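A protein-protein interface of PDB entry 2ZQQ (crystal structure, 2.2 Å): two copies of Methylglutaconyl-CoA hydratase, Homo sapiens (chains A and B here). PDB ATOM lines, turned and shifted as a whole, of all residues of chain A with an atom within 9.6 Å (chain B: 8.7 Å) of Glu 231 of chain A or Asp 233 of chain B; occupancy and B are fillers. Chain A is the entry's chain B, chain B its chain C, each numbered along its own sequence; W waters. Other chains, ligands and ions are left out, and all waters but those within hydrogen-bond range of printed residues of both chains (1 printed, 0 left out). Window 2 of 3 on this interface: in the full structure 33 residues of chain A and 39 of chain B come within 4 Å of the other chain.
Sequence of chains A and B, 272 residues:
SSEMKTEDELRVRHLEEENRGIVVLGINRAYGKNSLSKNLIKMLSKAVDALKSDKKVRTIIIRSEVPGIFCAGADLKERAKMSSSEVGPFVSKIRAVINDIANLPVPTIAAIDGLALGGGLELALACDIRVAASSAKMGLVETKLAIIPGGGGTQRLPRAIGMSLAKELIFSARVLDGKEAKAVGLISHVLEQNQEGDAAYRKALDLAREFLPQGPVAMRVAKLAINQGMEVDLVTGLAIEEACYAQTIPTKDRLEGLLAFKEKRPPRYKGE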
ATOM      1  N   ASN A  99      27.984  26.823 -16.011  1.00  0.00           N
ATOM      2  CA  ASN A  99      27.639  26.118 -17.246  1.00  0.00           C
ATOM      3  C   ASN A  99      26.332  25.339 -17.040  1.00  0.00           C
ATOM      4  O   ASN A  99      25.570  25.150 -17.984  1.00  0.00           O
ATOM      5  CB  ASN A  99      28.749  25.152 -17.692  1.00  0.00           C
ATOM      6  CG  ASN A  99      28.509  24.609 -19.106  1.00  0.00           C
ATOM      7  OD1 ASN A  99      28.376  25.373 -20.065  1.00  0.00           O
ATOM      8  ND2 ASN A  99      28.444  23.295 -19.235  1.00  0.00           N
ATOM      9  N   ALA A 102      23.638  27.693 -17.657  1.00  0.00           N
ATOM     10  CA  ALA A 102      23.510  27.876 -19.097  1.00  0.00           C
ATOM     11  C   ALA A 102      22.707  26.743 -19.736  1.00  0.00           C
ATOM     12  O   ALA A 102      22.065  26.945 -20.766  1.00  0.00           O
ATOM     13  CB  ALA A 102      24.911  27.966 -19.754  1.00  0.00           C
ATOM     14  N   ASN A 103      22.749  25.554 -19.138  1.00  0.00           N
ATOM     15  CA  ASN A 103      22.016  24.413 -19.688  1.00  0.00           C
ATOM     16  C   ASN A 103      20.635  24.160 -19.052  1.00  0.00           C
ATOM     17  O   ASN A 103      20.056  23.084 -19.242  1.00  0.00           O
ATOM     18  CB  ASN A 103      22.858  23.131 -19.599  1.00  0.00           C
ATOM     19  CG  ASN A 103      24.114  23.182 -20.481  1.00  0.00           C
ATOM     20  OD1 ASN A 103      24.067  23.610 -21.634  1.00  0.00           O
ATOM     21  ND2 ASN A 103      25.234  22.731 -19.936  1.00  0.00           N
ATOM     22  N   GLN A 155      34.812  32.882 -22.966  1.00  0.00           N
ATOM     23  CA  GLN A 155      34.040  32.137 -23.955  1.00  0.00           C
ATOM     24  C   GLN A 155      32.683  32.738 -24.282  1.00  0.00           C
ATOM     25  O   GLN A 155      32.332  32.864 -25.455  1.00  0.00           O
ATOM     26  CB  GLN A 155      33.840  30.690 -23.491  1.00  0.00           C
ATOM     27  CG  GLN A 155      35.131  29.943 -23.328  1.00  0.00           C
ATOM     28  CD  GLN A 155      36.034  30.090 -24.534  1.00  0.00           C
ATOM     29  OE1 GLN A 155      35.675  29.689 -25.643  1.00  0.00           O
ATOM     30  NE2 GLN A 155      37.220  30.669 -24.324  1.00  0.00           N
ATOM     31  N   ARG A 156      31.924  33.108 -23.253  1.00  0.00           N
ATOM     32  CA  ARG A 156      30.591  33.664 -23.469  1.00  0.00           C
ATOM     33  C   ARG A 156      30.499  35.138 -23.877  1.00  0.00           C
ATOM     34  O   ARG A 156      29.654  35.489 -24.698  1.00  0.00           O
ATOM     35  CB  ARG A 156      29.717  33.418 -22.233  1.00  0.00           C
ATOM     36  CG  ARG A 156      29.443  31.938 -21.983  1.00  0.00           C
ATOM     37  CD  ARG A 156      28.279  31.714 -21.031  1.00  0.00           C
ATOM     38  NE  ARG A 156      27.956  30.297 -20.941  1.00  0.00           N
ATOM     39  CZ  ARG A 156      28.576  29.441 -20.139  1.00  0.00           C
ATOM     40  NH1 ARG A 156      29.548  29.860 -19.343  1.00  0.00           N
ATOM     41  NH2 ARG A 156      28.251  28.163 -20.159  1.00  0.00           N
ATOM     42  N   ARG A 159      31.020  35.454 -27.581  1.00  0.00           N
ATOM     43  CA  ARG A 159      29.910  34.885 -28.326  1.00  0.00           C
ATOM     44  C   ARG A 159      28.675  35.775 -28.218  1.00  0.00           C
ATOM     45  O   ARG A 159      27.772  35.679 -29.031  1.00  0.00           O
ATOM     46  CB  ARG A 159      29.585  33.475 -27.814  1.00  0.00           C
ATOM     47  CG  ARG A 159      30.655  32.459 -28.130  1.00  0.00           C
ATOM     48  CD  ARG A 159      30.346  31.106 -27.529  1.00  0.00           C
ATOM     49  NE  ARG A 159      31.123  30.039 -28.160  1.00  0.00           N
ATOM     50  CZ  ARG A 159      32.424  29.831 -27.985  1.00  0.00           C
ATOM     51  NH1 ARG A 159      33.138  30.613 -27.189  1.00  0.00           N
ATOM     52  NH2 ARG A 159      33.014  28.824 -28.602  1.00  0.00           N
ATOM     53  N   LYS A 223      14.553  26.074 -27.138  1.00  0.00           N
ATOM     54  CA  LYS A 223      15.810  26.460 -26.507  1.00  0.00           C
ATOM     55  C   LYS A 223      16.889  25.432 -26.876  1.00  0.00           C
ATOM     56  O   LYS A 223      18.029  25.782 -27.194  1.00  0.00           O
ATOM     57  CB  LYS A 223      15.652  26.535 -24.985  1.00  0.00           C
ATOM     58  CG  LYS A 223      16.947  26.914 -24.274  1.00  0.00           C
ATOM     59  CD  LYS A 223      16.749  27.262 -22.806  1.00  0.00           C
ATOM     60  CE  LYS A 223      18.068  27.744 -22.206  1.00  0.00           C
ATOM     61  NZ  LYS A 223      17.876  28.425 -20.902  1.00  0.00           N
ATOM     62  N   LEU A 224      16.506  24.163 -26.837  1.00  0.00           N
ATOM     63  CA  LEU A 224      17.398  23.076 -27.183  1.00  0.00           C
ATOM     64  C   LEU A 224      17.923  23.252 -28.618  1.00  0.00           C
ATOM     65  O   LEU A 224      19.132  23.178 -28.871  1.00  0.00           O
ATOM     66  CB  LEU A 224      16.641  21.747 -27.078  1.00  0.00           C
ATOM     67  CG  LEU A 224      17.464  20.474 -26.892  1.00  0.00           C
ATOM     68  CD1 LEU A 224      18.021  20.462 -25.469  1.00  0.00           C
ATOM     69  CD2 LEU A 224      16.588  19.235 -27.114  1.00  0.00           C
ATOM     70  N   ALA A 225      17.009  23.477 -29.557  1.00  0.00           N
ATOM     71  CA  ALA A 225      17.376  23.644 -30.964  1.00  0.00           C
ATOM     72  C   ALA A 225      18.314  24.823 -31.189  1.00  0.00           C
ATOM     73  O   ALA A 225      19.262  24.732 -31.973  1.00  0.00           O
ATOM     74  CB  ALA A 225      16.118  23.805 -31.819  1.00  0.00           C
ATOM     75  N   ILE A 226      18.051  25.933 -30.508  1.00  0.00           N
ATOM     76  CA  ILE A 226      18.886  27.121 -30.646  1.00  0.00           C
ATOM     77  C   ILE A 226      20.266  26.900 -30.028  1.00  0.00           C
ATOM     78  O   ILE A 226      21.287  27.162 -30.669  1.00  0.00           O
ATOM     79  CB  ILE A 226      18.214  28.343 -29.984  1.00  0.00           C
ATOM     80  CG1 ILE A 226      17.010  28.778 -30.821  1.00  0.00           C
ATOM     81  CG2 ILE A 226      19.213  29.489 -29.835  1.00  0.00           C
ATOM     82  CD1 ILE A 226      16.225  29.907 -30.209  1.00  0.00           C
ATOM     83  N   ASN A 227      20.297  26.407 -28.789  1.00  0.00           N
ATOM     84  CA  ASN A 227      21.562  26.172 -28.113  1.00  0.00           C
ATOM     85  C   ASN A 227      22.436  25.152 -28.823  1.00  0.00           C
ATOM     86  O   ASN A 227      23.607  25.424 -29.082  1.00  0.00           O
ATOM     87  CB  ASN A 227      21.330  25.731 -26.669  1.00  0.00           C
ATOM     88  CG  ASN A 227      21.246  26.897 -25.715  1.00  0.00           C
ATOM     89  OD1 ASN A 227      21.321  28.055 -26.127  1.00  0.00           O
ATOM     90  ND2 ASN A 227      21.093  26.604 -24.433  1.00  0.00           N
ATOM     91  N   GLN A 228      21.879  23.986 -29.144  1.00  0.00           N
ATOM     92  CA  GLN A 228      22.655  22.947 -29.820  1.00  0.00           C
ATOM     93  C   GLN A 228      22.895  23.340 -31.270  1.00  0.00           C
ATOM     94  O   GLN A 228      23.987  23.155 -31.797  1.00  0.00           O
ATOM     95  CB  GLN A 228      21.941  21.590 -29.747  1.00  0.00           C
ATOM     96  CG  GLN A 228      21.479  21.216 -28.328  1.00  0.00           C
ATOM     97  CD  GLN A 228      21.120  19.741 -28.166  1.00  0.00           C
ATOM     98  OE1 GLN A 228      20.672  19.084 -29.111  1.00  0.00           O
ATOM     99  NE2 GLN A 228      21.301  19.220 -26.953  1.00  0.00           N
ATOM    100  N   GLY A 229      21.879  23.902 -31.911  1.00  0.00           N
ATOM    101  CA  GLY A 229      22.035  24.310 -33.292  1.00  0.00           C
ATOM    102  C   GLY A 229      23.243  25.205 -33.516  1.00  0.00           C
ATOM    103  O   GLY A 229      23.947  25.069 -34.516  1.00  0.00           O
ATOM    104  N   MET A 230      23.486  26.118 -32.581  1.00  0.00           N
ATOM    105  CA  MET A 230      24.593  27.058 -32.695  1.00  0.00           C
ATOM    106  C   MET A 230      25.965  26.453 -32.441  1.00  0.00           C
ATOM    107  O   MET A 230      26.980  27.099 -32.717  1.00  0.00           O
ATOM    108  CB  MET A 230      24.390  28.250 -31.747  1.00  0.00           C
ATOM    109  CG  MET A 230      23.311  29.239 -32.171  1.00  0.00           C
ATOM    110  SD  MET A 230      23.661  30.085 -33.735  1.00  0.00           S
ATOM    111  CE  MET A 230      24.970  31.178 -33.229  1.00  0.00           C
ATOM    112  N   GLU A 231      26.007  25.227 -31.924  1.00  0.00           N
ATOM    113  CA  GLU A 231      27.287  24.581 -31.662  1.00  0.00           C
ATOM    114  C   GLU A 231      27.764  23.727 -32.840  1.00  0.00           C
ATOM    115  O   GLU A 231      28.908  23.279 -32.859  1.00  0.00           O
ATOM    116  CB  GLU A 231      27.213  23.714 -30.399  1.00  0.00           C
ATOM    117  CG  GLU A 231      26.996  24.485 -29.096  1.00  0.00           C
ATOM    118  CD  GLU A 231      28.046  25.556 -28.843  1.00  0.00           C
ATOM    119  OE1 GLU A 231      29.253  25.273 -29.014  1.00  0.00           O
ATOM    120  OE2 GLU A 231      27.666  26.684 -28.457  1.00  0.00           O
ATOM    121  N   VAL A 232      26.890  23.500 -33.816  1.00  0.00           N
ATOM    122  CA  VAL A 232      27.251  22.710 -34.991  1.00  0.00           C
ATOM    123  C   VAL A 232      27.032  23.496 -36.280  1.00  0.00           C
ATOM    124  O   VAL A 232      26.485  24.603 -36.255  1.00  0.00           O
ATOM    125  CB  VAL A 232      26.422  21.415 -35.067  1.00  0.00           C
ATOM    126  CG1 VAL A 232      26.709  20.550 -33.849  1.00  0.00           C
ATOM    127  CG2 VAL A 232      24.929  21.750 -35.161  1.00  0.00           C
ATOM    128  N   ASP A 233      27.458  22.926 -37.404  1.00  0.00           N
ATOM    129  CA  ASP A 233      27.288  23.583 -38.700  1.00  0.00           C
ATOM    130  C   ASP A 233      25.800  23.677 -39.022  1.00  0.00           C
ATOM    131  O   ASP A 233      24.999  22.895 -38.515  1.00  0.00           O
ATOM    132  CB  ASP A 233      27.992  22.795 -39.797  1.00  0.00           C
ATOM    133  CG  ASP A 233      27.476  21.386 -39.908  1.00  0.00           C
ATOM    134  OD1 ASP A 233      27.841  20.551 -39.057  1.00  0.00           O
ATOM    135  OD2 ASP A 233      26.690  21.115 -40.838  1.00  0.00           O
ATOM    136  N   LEU A 234      25.440  24.615 -39.889  1.00  0.00           N
ATOM    137  CA  LEU A 234      24.044  24.836 -40.243  1.00  0.00           C
ATOM    138  C   LEU A 234      23.250  23.602 -40.677  1.00  0.00           C
ATOM    139  O   LEU A 234      22.129  23.391 -40.198  1.00  0.00           O
ATOM    140  CB  LEU A 234      23.938  25.930 -41.310  1.00  0.00           C
ATOM    141  CG  LEU A 234      22.516  26.378 -41.669  1.00  0.00           C
ATOM    142  CD1 LEU A 234      21.678  26.577 -40.412  1.00  0.00           C
ATOM    143  CD2 LEU A 234      22.591  27.677 -42.470  1.00  0.00           C
ATOM    144  N   THR A 236      23.650  20.464 -39.939  1.00  0.00           N
ATOM    145  CA  THR A 236      23.370  19.640 -38.774  1.00  0.00           C
ATOM    146  C   THR A 236      22.347  20.349 -37.888  1.00  0.00           C
ATOM    147  O   THR A 236      21.495  19.710 -37.282  1.00  0.00           O
ATOM    148  CB  THR A 236      24.656  19.360 -37.957  1.00  0.00           C
ATOM    149  OG1 THR A 236      25.619  18.711 -38.792  1.00  0.00           O
ATOM    150  CG2 THR A 236      24.352  18.444 -36.777  1.00  0.00           C
ATOM    151  N   GLY A 237      22.438  21.675 -37.824  1.00  0.00           N
ATOM    152  CA  GLY A 237      21.510  22.458 -37.022  1.00  0.00           C
ATOM    153  C   GLY A 237      20.089  22.312 -37.520  1.00  0.00           C
ATOM    154  O   GLY A 237      19.142  22.286 -36.725  1.00  0.00           O
ATOM    155  N   ILE A 240      18.757  19.124 -36.407  1.00  0.00           N
ATOM    156  CA  ILE A 240      18.425  19.219 -34.993  1.00  0.00           C
ATOM    157  C   ILE A 240      17.079  19.914 -34.834  1.00  0.00           C
ATOM    158  O   ILE A 240      16.269  19.520 -33.992  1.00  0.00           O
ATOM    159  CB  ILE A 240      19.534  19.954 -34.207  1.00  0.00           C
ATOM    160  CG1 ILE A 240      20.759  19.034 -34.094  1.00  0.00           C
ATOM    161  CG2 ILE A 240      19.037  20.356 -32.825  1.00  0.00           C
ATOM    162  CD1 ILE A 240      21.948  19.650 -33.384  1.00  0.00           C
ATOM    163  N   GLN B 228      41.328  31.060 -29.544  1.00  0.00           N
ATOM    164  CA  GLN B 228      41.170  29.622 -29.743  1.00  0.00           C
ATOM    165  C   GLN B 228      39.791  29.101 -29.348  1.00  0.00           C
ATOM    166  O   GLN B 228      39.259  28.200 -29.992  1.00  0.00           O
ATOM    167  CB  GLN B 228      42.268  28.859 -28.995  1.00  0.00           C
ATOM    168  CG  GLN B 228      43.609  28.923 -29.709  1.00  0.00           C
ATOM    169  CD  GLN B 228      44.711  28.208 -28.961  1.00  0.00           C
ATOM    170  OE1 GLN B 228      44.458  27.372 -28.086  1.00  0.00           O
ATOM    171  NE2 GLN B 228      45.951  28.522 -29.312  1.00  0.00           N
ATOM    172  N   GLY B 229      39.197  29.685 -28.316  1.00  0.00           N
ATOM    173  CA  GLY B 229      37.882  29.237 -27.880  1.00  0.00           C
ATOM    174  C   GLY B 229      36.792  29.482 -28.908  1.00  0.00           C
ATOM    175  O   GLY B 229      35.834  28.709 -29.016  1.00  0.00           O
ATOM    176  N   MET B 230      36.930  30.562 -29.667  1.00  0.00           N
ATOM    177  CA  MET B 230      35.942  30.898 -30.684  1.00  0.00           C
ATOM    178  C   MET B 230      36.065  30.035 -31.945  1.00  0.00           C
ATOM    179  O   MET B 230      35.207  30.093 -32.818  1.00  0.00           O
ATOM    180  CB  MET B 230      36.042  32.391 -31.052  1.00  0.00           C
ATOM    181  CG  MET B 230      35.513  33.354 -29.975  1.00  0.00           C
ATOM    182  SD  MET B 230      33.721  33.198 -29.639  1.00  0.00           S
ATOM    183  CE  MET B 230      33.063  33.793 -31.220  1.00  0.00           C
ATOM    184  N   GLU B 231      37.124  29.232 -32.036  1.00  0.00           N
ATOM    185  CA  GLU B 231      37.320  28.356 -33.193  1.00  0.00           C
ATOM    186  C   GLU B 231      36.801  26.942 -32.943  1.00  0.00           C
ATOM    187  O   GLU B 231      36.860  26.086 -33.827  1.00  0.00           O
ATOM    188  CB  GLU B 231      38.799  28.292 -33.573  1.00  0.00           C
ATOM    189  CG  GLU B 231      39.363  29.617 -34.068  1.00  0.00           C
ATOM    190  CD  GLU B 231      38.503  30.249 -35.153  1.00  0.00           C
ATOM    191  OE1 GLU B 231      38.062  29.519 -36.065  1.00  0.00           O
ATOM    192  OE2 GLU B 231      38.275  31.480 -35.100  1.00  0.00           O
ATOM    193  N   VAL B 232      36.305  26.697 -31.730  1.00  0.00           N
ATOM    194  CA  VAL B 232      35.761  25.391 -31.372  1.00  0.00           C
ATOM    195  C   VAL B 232      34.408  25.581 -30.697  1.00  0.00           C
ATOM    196  O   VAL B 232      33.942  26.713 -30.529  1.00  0.00           O
ATOM    197  CB  VAL B 232      36.692  24.618 -30.401  1.00  0.00           C
ATOM    198  CG1 VAL B 232      38.019  24.297 -31.095  1.00  0.00           C
ATOM    199  CG2 VAL B 232      36.932  25.452 -29.131  1.00  0.00           C
ATOM    200  N   ASP B 233      33.782  24.473 -30.313  1.00  0.00           N
ATOM    201  CA  ASP B 233      32.489  24.530 -29.653  1.00  0.00           C
ATOM    202  C   ASP B 233      32.712  25.035 -28.228  1.00  0.00           C
ATOM    203  O   ASP B 233      33.846  25.045 -27.723  1.00  0.00           O
ATOM    204  CB  ASP B 233      31.825  23.142 -29.664  1.00  0.00           C
ATOM    205  CG  ASP B 233      32.637  22.101 -28.924  1.00  0.00           C
ATOM    206  OD1 ASP B 233      32.774  22.220 -27.694  1.00  0.00           O
ATOM    207  OD2 ASP B 233      33.150  21.168 -29.565  1.00  0.00           O
ATOM    208  N   LEU B 234      31.633  25.469 -27.592  1.00  0.00           N
ATOM    209  CA  LEU B 234      31.708  26.022 -26.244  1.00  0.00           C
ATOM    210  C   LEU B 234      32.291  25.087 -25.171  1.00  0.00           C
ATOM    211  O   LEU B 234      33.069  25.525 -24.323  1.00  0.00           O
ATOM    212  CB  LEU B 234      30.320  26.520 -25.840  1.00  0.00           C
ATOM    213  CG  LEU B 234      30.144  27.317 -24.547  1.00  0.00           C
ATOM    214  CD1 LEU B 234      31.268  28.322 -24.361  1.00  0.00           C
ATOM    215  CD2 LEU B 234      28.799  28.031 -24.618  1.00  0.00           C
ATOM    216  N   VAL B 235      31.933  23.809 -25.197  1.00  0.00           N
ATOM    217  CA  VAL B 235      32.464  22.885 -24.202  1.00  0.00           C
ATOM    218  C   VAL B 235      33.987  22.841 -24.310  1.00  0.00           C
ATOM    219  O   VAL B 235      34.681  22.924 -23.309  1.00  0.00           O
ATOM    220  CB  VAL B 235      31.875  21.460 -24.369  1.00  0.00           C
ATOM    221  CG1 VAL B 235      32.577  20.496 -23.434  1.00  0.00           C
ATOM    222  CG2 VAL B 235      30.381  21.470 -24.036  1.00  0.00           C
ATOM    223  N   THR B 236      34.510  22.720 -25.525  1.00  0.00           N
ATOM    224  CA  THR B 236      35.956  22.697 -25.710  1.00  0.00           C
ATOM    225  C   THR B 236      36.499  24.071 -25.322  1.00  0.00           C
ATOM    226  O   THR B 236      37.588  24.195 -24.752  1.00  0.00           O
ATOM    227  CB  THR B 236      36.330  22.386 -27.175  1.00  0.00           C
ATOM    228  OG1 THR B 236      35.774  21.120 -27.547  1.00  0.00           O
ATOM    229  CG2 THR B 236      37.849  22.302 -27.340  1.00  0.00           C
ATOM    230  N   GLY B 237      35.719  25.103 -25.630  1.00  0.00           N
ATOM    231  CA  GLY B 237      36.118  26.457 -25.294  1.00  0.00           C
ATOM    232  C   GLY B 237      36.311  26.604 -23.798  1.00  0.00           C
ATOM    233  O   GLY B 237      37.278  27.221 -23.362  1.00  0.00           O
ATOM    234  N   LEU B 238      35.399  26.034 -23.010  1.00  0.00           N
ATOM    235  CA  LEU B 238      35.508  26.113 -21.558  1.00  0.00           C
ATOM    236  C   LEU B 238      36.776  25.415 -21.053  1.00  0.00           C
ATOM    237  O   LEU B 238      37.408  25.876 -20.102  1.00  0.00           O
ATOM    238  CB  LEU B 238      34.250  25.514 -20.903  1.00  0.00           C
ATOM    239  CG  LEU B 238      32.974  26.349 -21.139  1.00  0.00           C
ATOM    240  CD1 LEU B 238      31.759  25.594 -20.663  1.00  0.00           C
ATOM    241  CD2 LEU B 238      33.074  27.690 -20.419  1.00  0.00           C
ATOM    242  N   ALA B 239      37.165  24.313 -21.691  1.00  0.00           N
ATOM    243  CA  ALA B 239      38.373  23.611 -21.278  1.00  0.00           C
ATOM    244  C   ALA B 239      39.597  24.473 -21.600  1.00  0.00           C
ATOM    245  O   ALA B 239      40.571  24.475 -20.851  1.00  0.00           O
ATOM    246  CB  ALA B 239      38.475  22.246 -21.986  1.00  0.00           C
ATOM    247  N   ILE B 240      39.538  25.212 -22.705  1.00  0.00           N
ATOM    248  CA  ILE B 240      40.647  26.080 -23.101  1.00  0.00           C
ATOM    249  C   ILE B 240      40.794  27.217 -22.082  1.00  0.00           C
ATOM    250  O   ILE B 240      41.901  27.587 -21.696  1.00  0.00           O
ATOM    251  CB  ILE B 240      40.419  26.662 -24.516  1.00  0.00           C
ATOM    252  CG1 ILE B 240      40.532  25.537 -25.557  1.00  0.00           C
ATOM    253  CG2 ILE B 240      41.426  27.802 -24.793  1.00  0.00           C
ATOM    254  CD1 ILE B 240      40.251  25.988 -27.008  1.00  0.00           C
HETATM  255  O   HOH W   1      29.479  23.250 -26.719  1.00  0.00           O
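The guanidinium group (NH2) of Arg 159 of chain A sits at hydrogen-bond distance from the backbone carbonyl oxygen (O) of Gly 229 of chain B, 2.9 Å away. The side-chain sulfur (SD) of Met 230 of chain B lies close to the guanidinium group (NH1) of Arg 159 of chain A, 3.6 Å away. NH2 of Arg 159 of chain A sits at hydrogen-bond distance from O of Val 232 of chain B (3.0 Å). N of Leu 234 of chain B sits at hydrogen-bond distance from OE1 of Glu 231 of chain A (2.8 Å).
O of Asn 99 of chain A lies within hydrogen-bond range of ND2 of Asn 103 of chain A, at 3.1 Å. The guanidinium group (NH2) of Arg 156 of chain A sits at hydrogen-bond distance from the side-chain amide oxygen (OD1) of Asn 99 of chain A. NH1 of Arg 159 of chain A lies within hydrogen-bond range of O of Gln 155 of chain A (3.0 Å). OD1 of Asp 233 of chain B sits at hydrogen-bond distance from N of Val 235 of chain B, 3.1 Å away. N of Thr 236 of chain B is in hydrogen-bond range of OD1 of Asp 233 of chain B (2.8 Å).
Among the printed residues, merely in contact across the chains: Gln 155 of chain A with Gly 229 of chain B, Gln 155 of chain A with Gly 237 of chain B, Glu 231 of chain A with Asp 233 of chain B, Asn 99 of chain A with Leu 238 of chain B, Gln 155 of chain A with Leu 234 of chain B, Arg 159 of chain A with Leu 234 of chain B, Arg 159 of chain A with Asp 233 of chain B and Gln 155 of chain A with Leu 238 of chain B.
Of the printed residues of chain B, Glu 231 of chain A touches Asp 233 (3.4 Å) and Leu 234 (2.8 Å). Of chain A, only Arg 159 and Glu 231 come within 4 Å of Asp 233 of chain B. No residue of chain B comes within 4 Å of Val 232 of chain A. Leu 234 of chain B touches just these residues of chain A: Gln 155, Arg 159 and Glu 231. No residue of chain A comes within 4 Å of Val 235 of chain B. No residue of chain A comes within 4 Å of Thr 236 of chain B. Printed residues of chain A within 4 Å of Met 230 of chain B: Arg 159. Printed residues of chain B within 4 Å of Gln 155 of chain A: Gly 229, Leu 234, Gly 237 and Leu 238. The nearest residue of chain B that does not touch Glu 231 of chain A is Val 235 of chain B (4.9 Å). The nearest printed residue of chain B that does not touch Asn 99 of chain A is Leu 234 of chain B (5.2 Å).
Of the 21 printed residues of chain A, 4 touch a printed residue of chain B. Printed residues of chain A that touch a printed residue of chain B: Asn 99, Gln 155, Arg 159 and Glu 231. Of the 13 printed residues of chain B, 7 touch a printed residue of chain A. Printed residues of chain B that touch a printed residue of chain A: Gly 229, Met 230, Val 232, Asp 233, Leu 234, Gly 237 and Leu 238. Among the printed residues, 12 pairs touch across the chains. Among the printed residues, no Asp or Glu carboxylate lies within 4 Å of a Lys or Arg side-chain nitrogen of the other chain.
Glu 231 of chain A touches Asp 233 of chain B, but with the chains exchanged Asp 233 of chain A does not touch Glu 231 of chain B (10.5 Å). Glu 231 of chain A touches Leu 234 of chain B, but with the chains exchanged Leu 234 of chain A does not touch Glu 231 of chain B (13.0 Å). Positions printed for both chains: 228, 229, 230, 231, 232, 233, 234, 236, 237 and 240.
Water W1 lies within hydrogen-bond range of the backbone NH of Val 235 of chain B, the side-chain carboxylate of Glu 231 of chain A and the backbone NH of Leu 234 of chain B.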
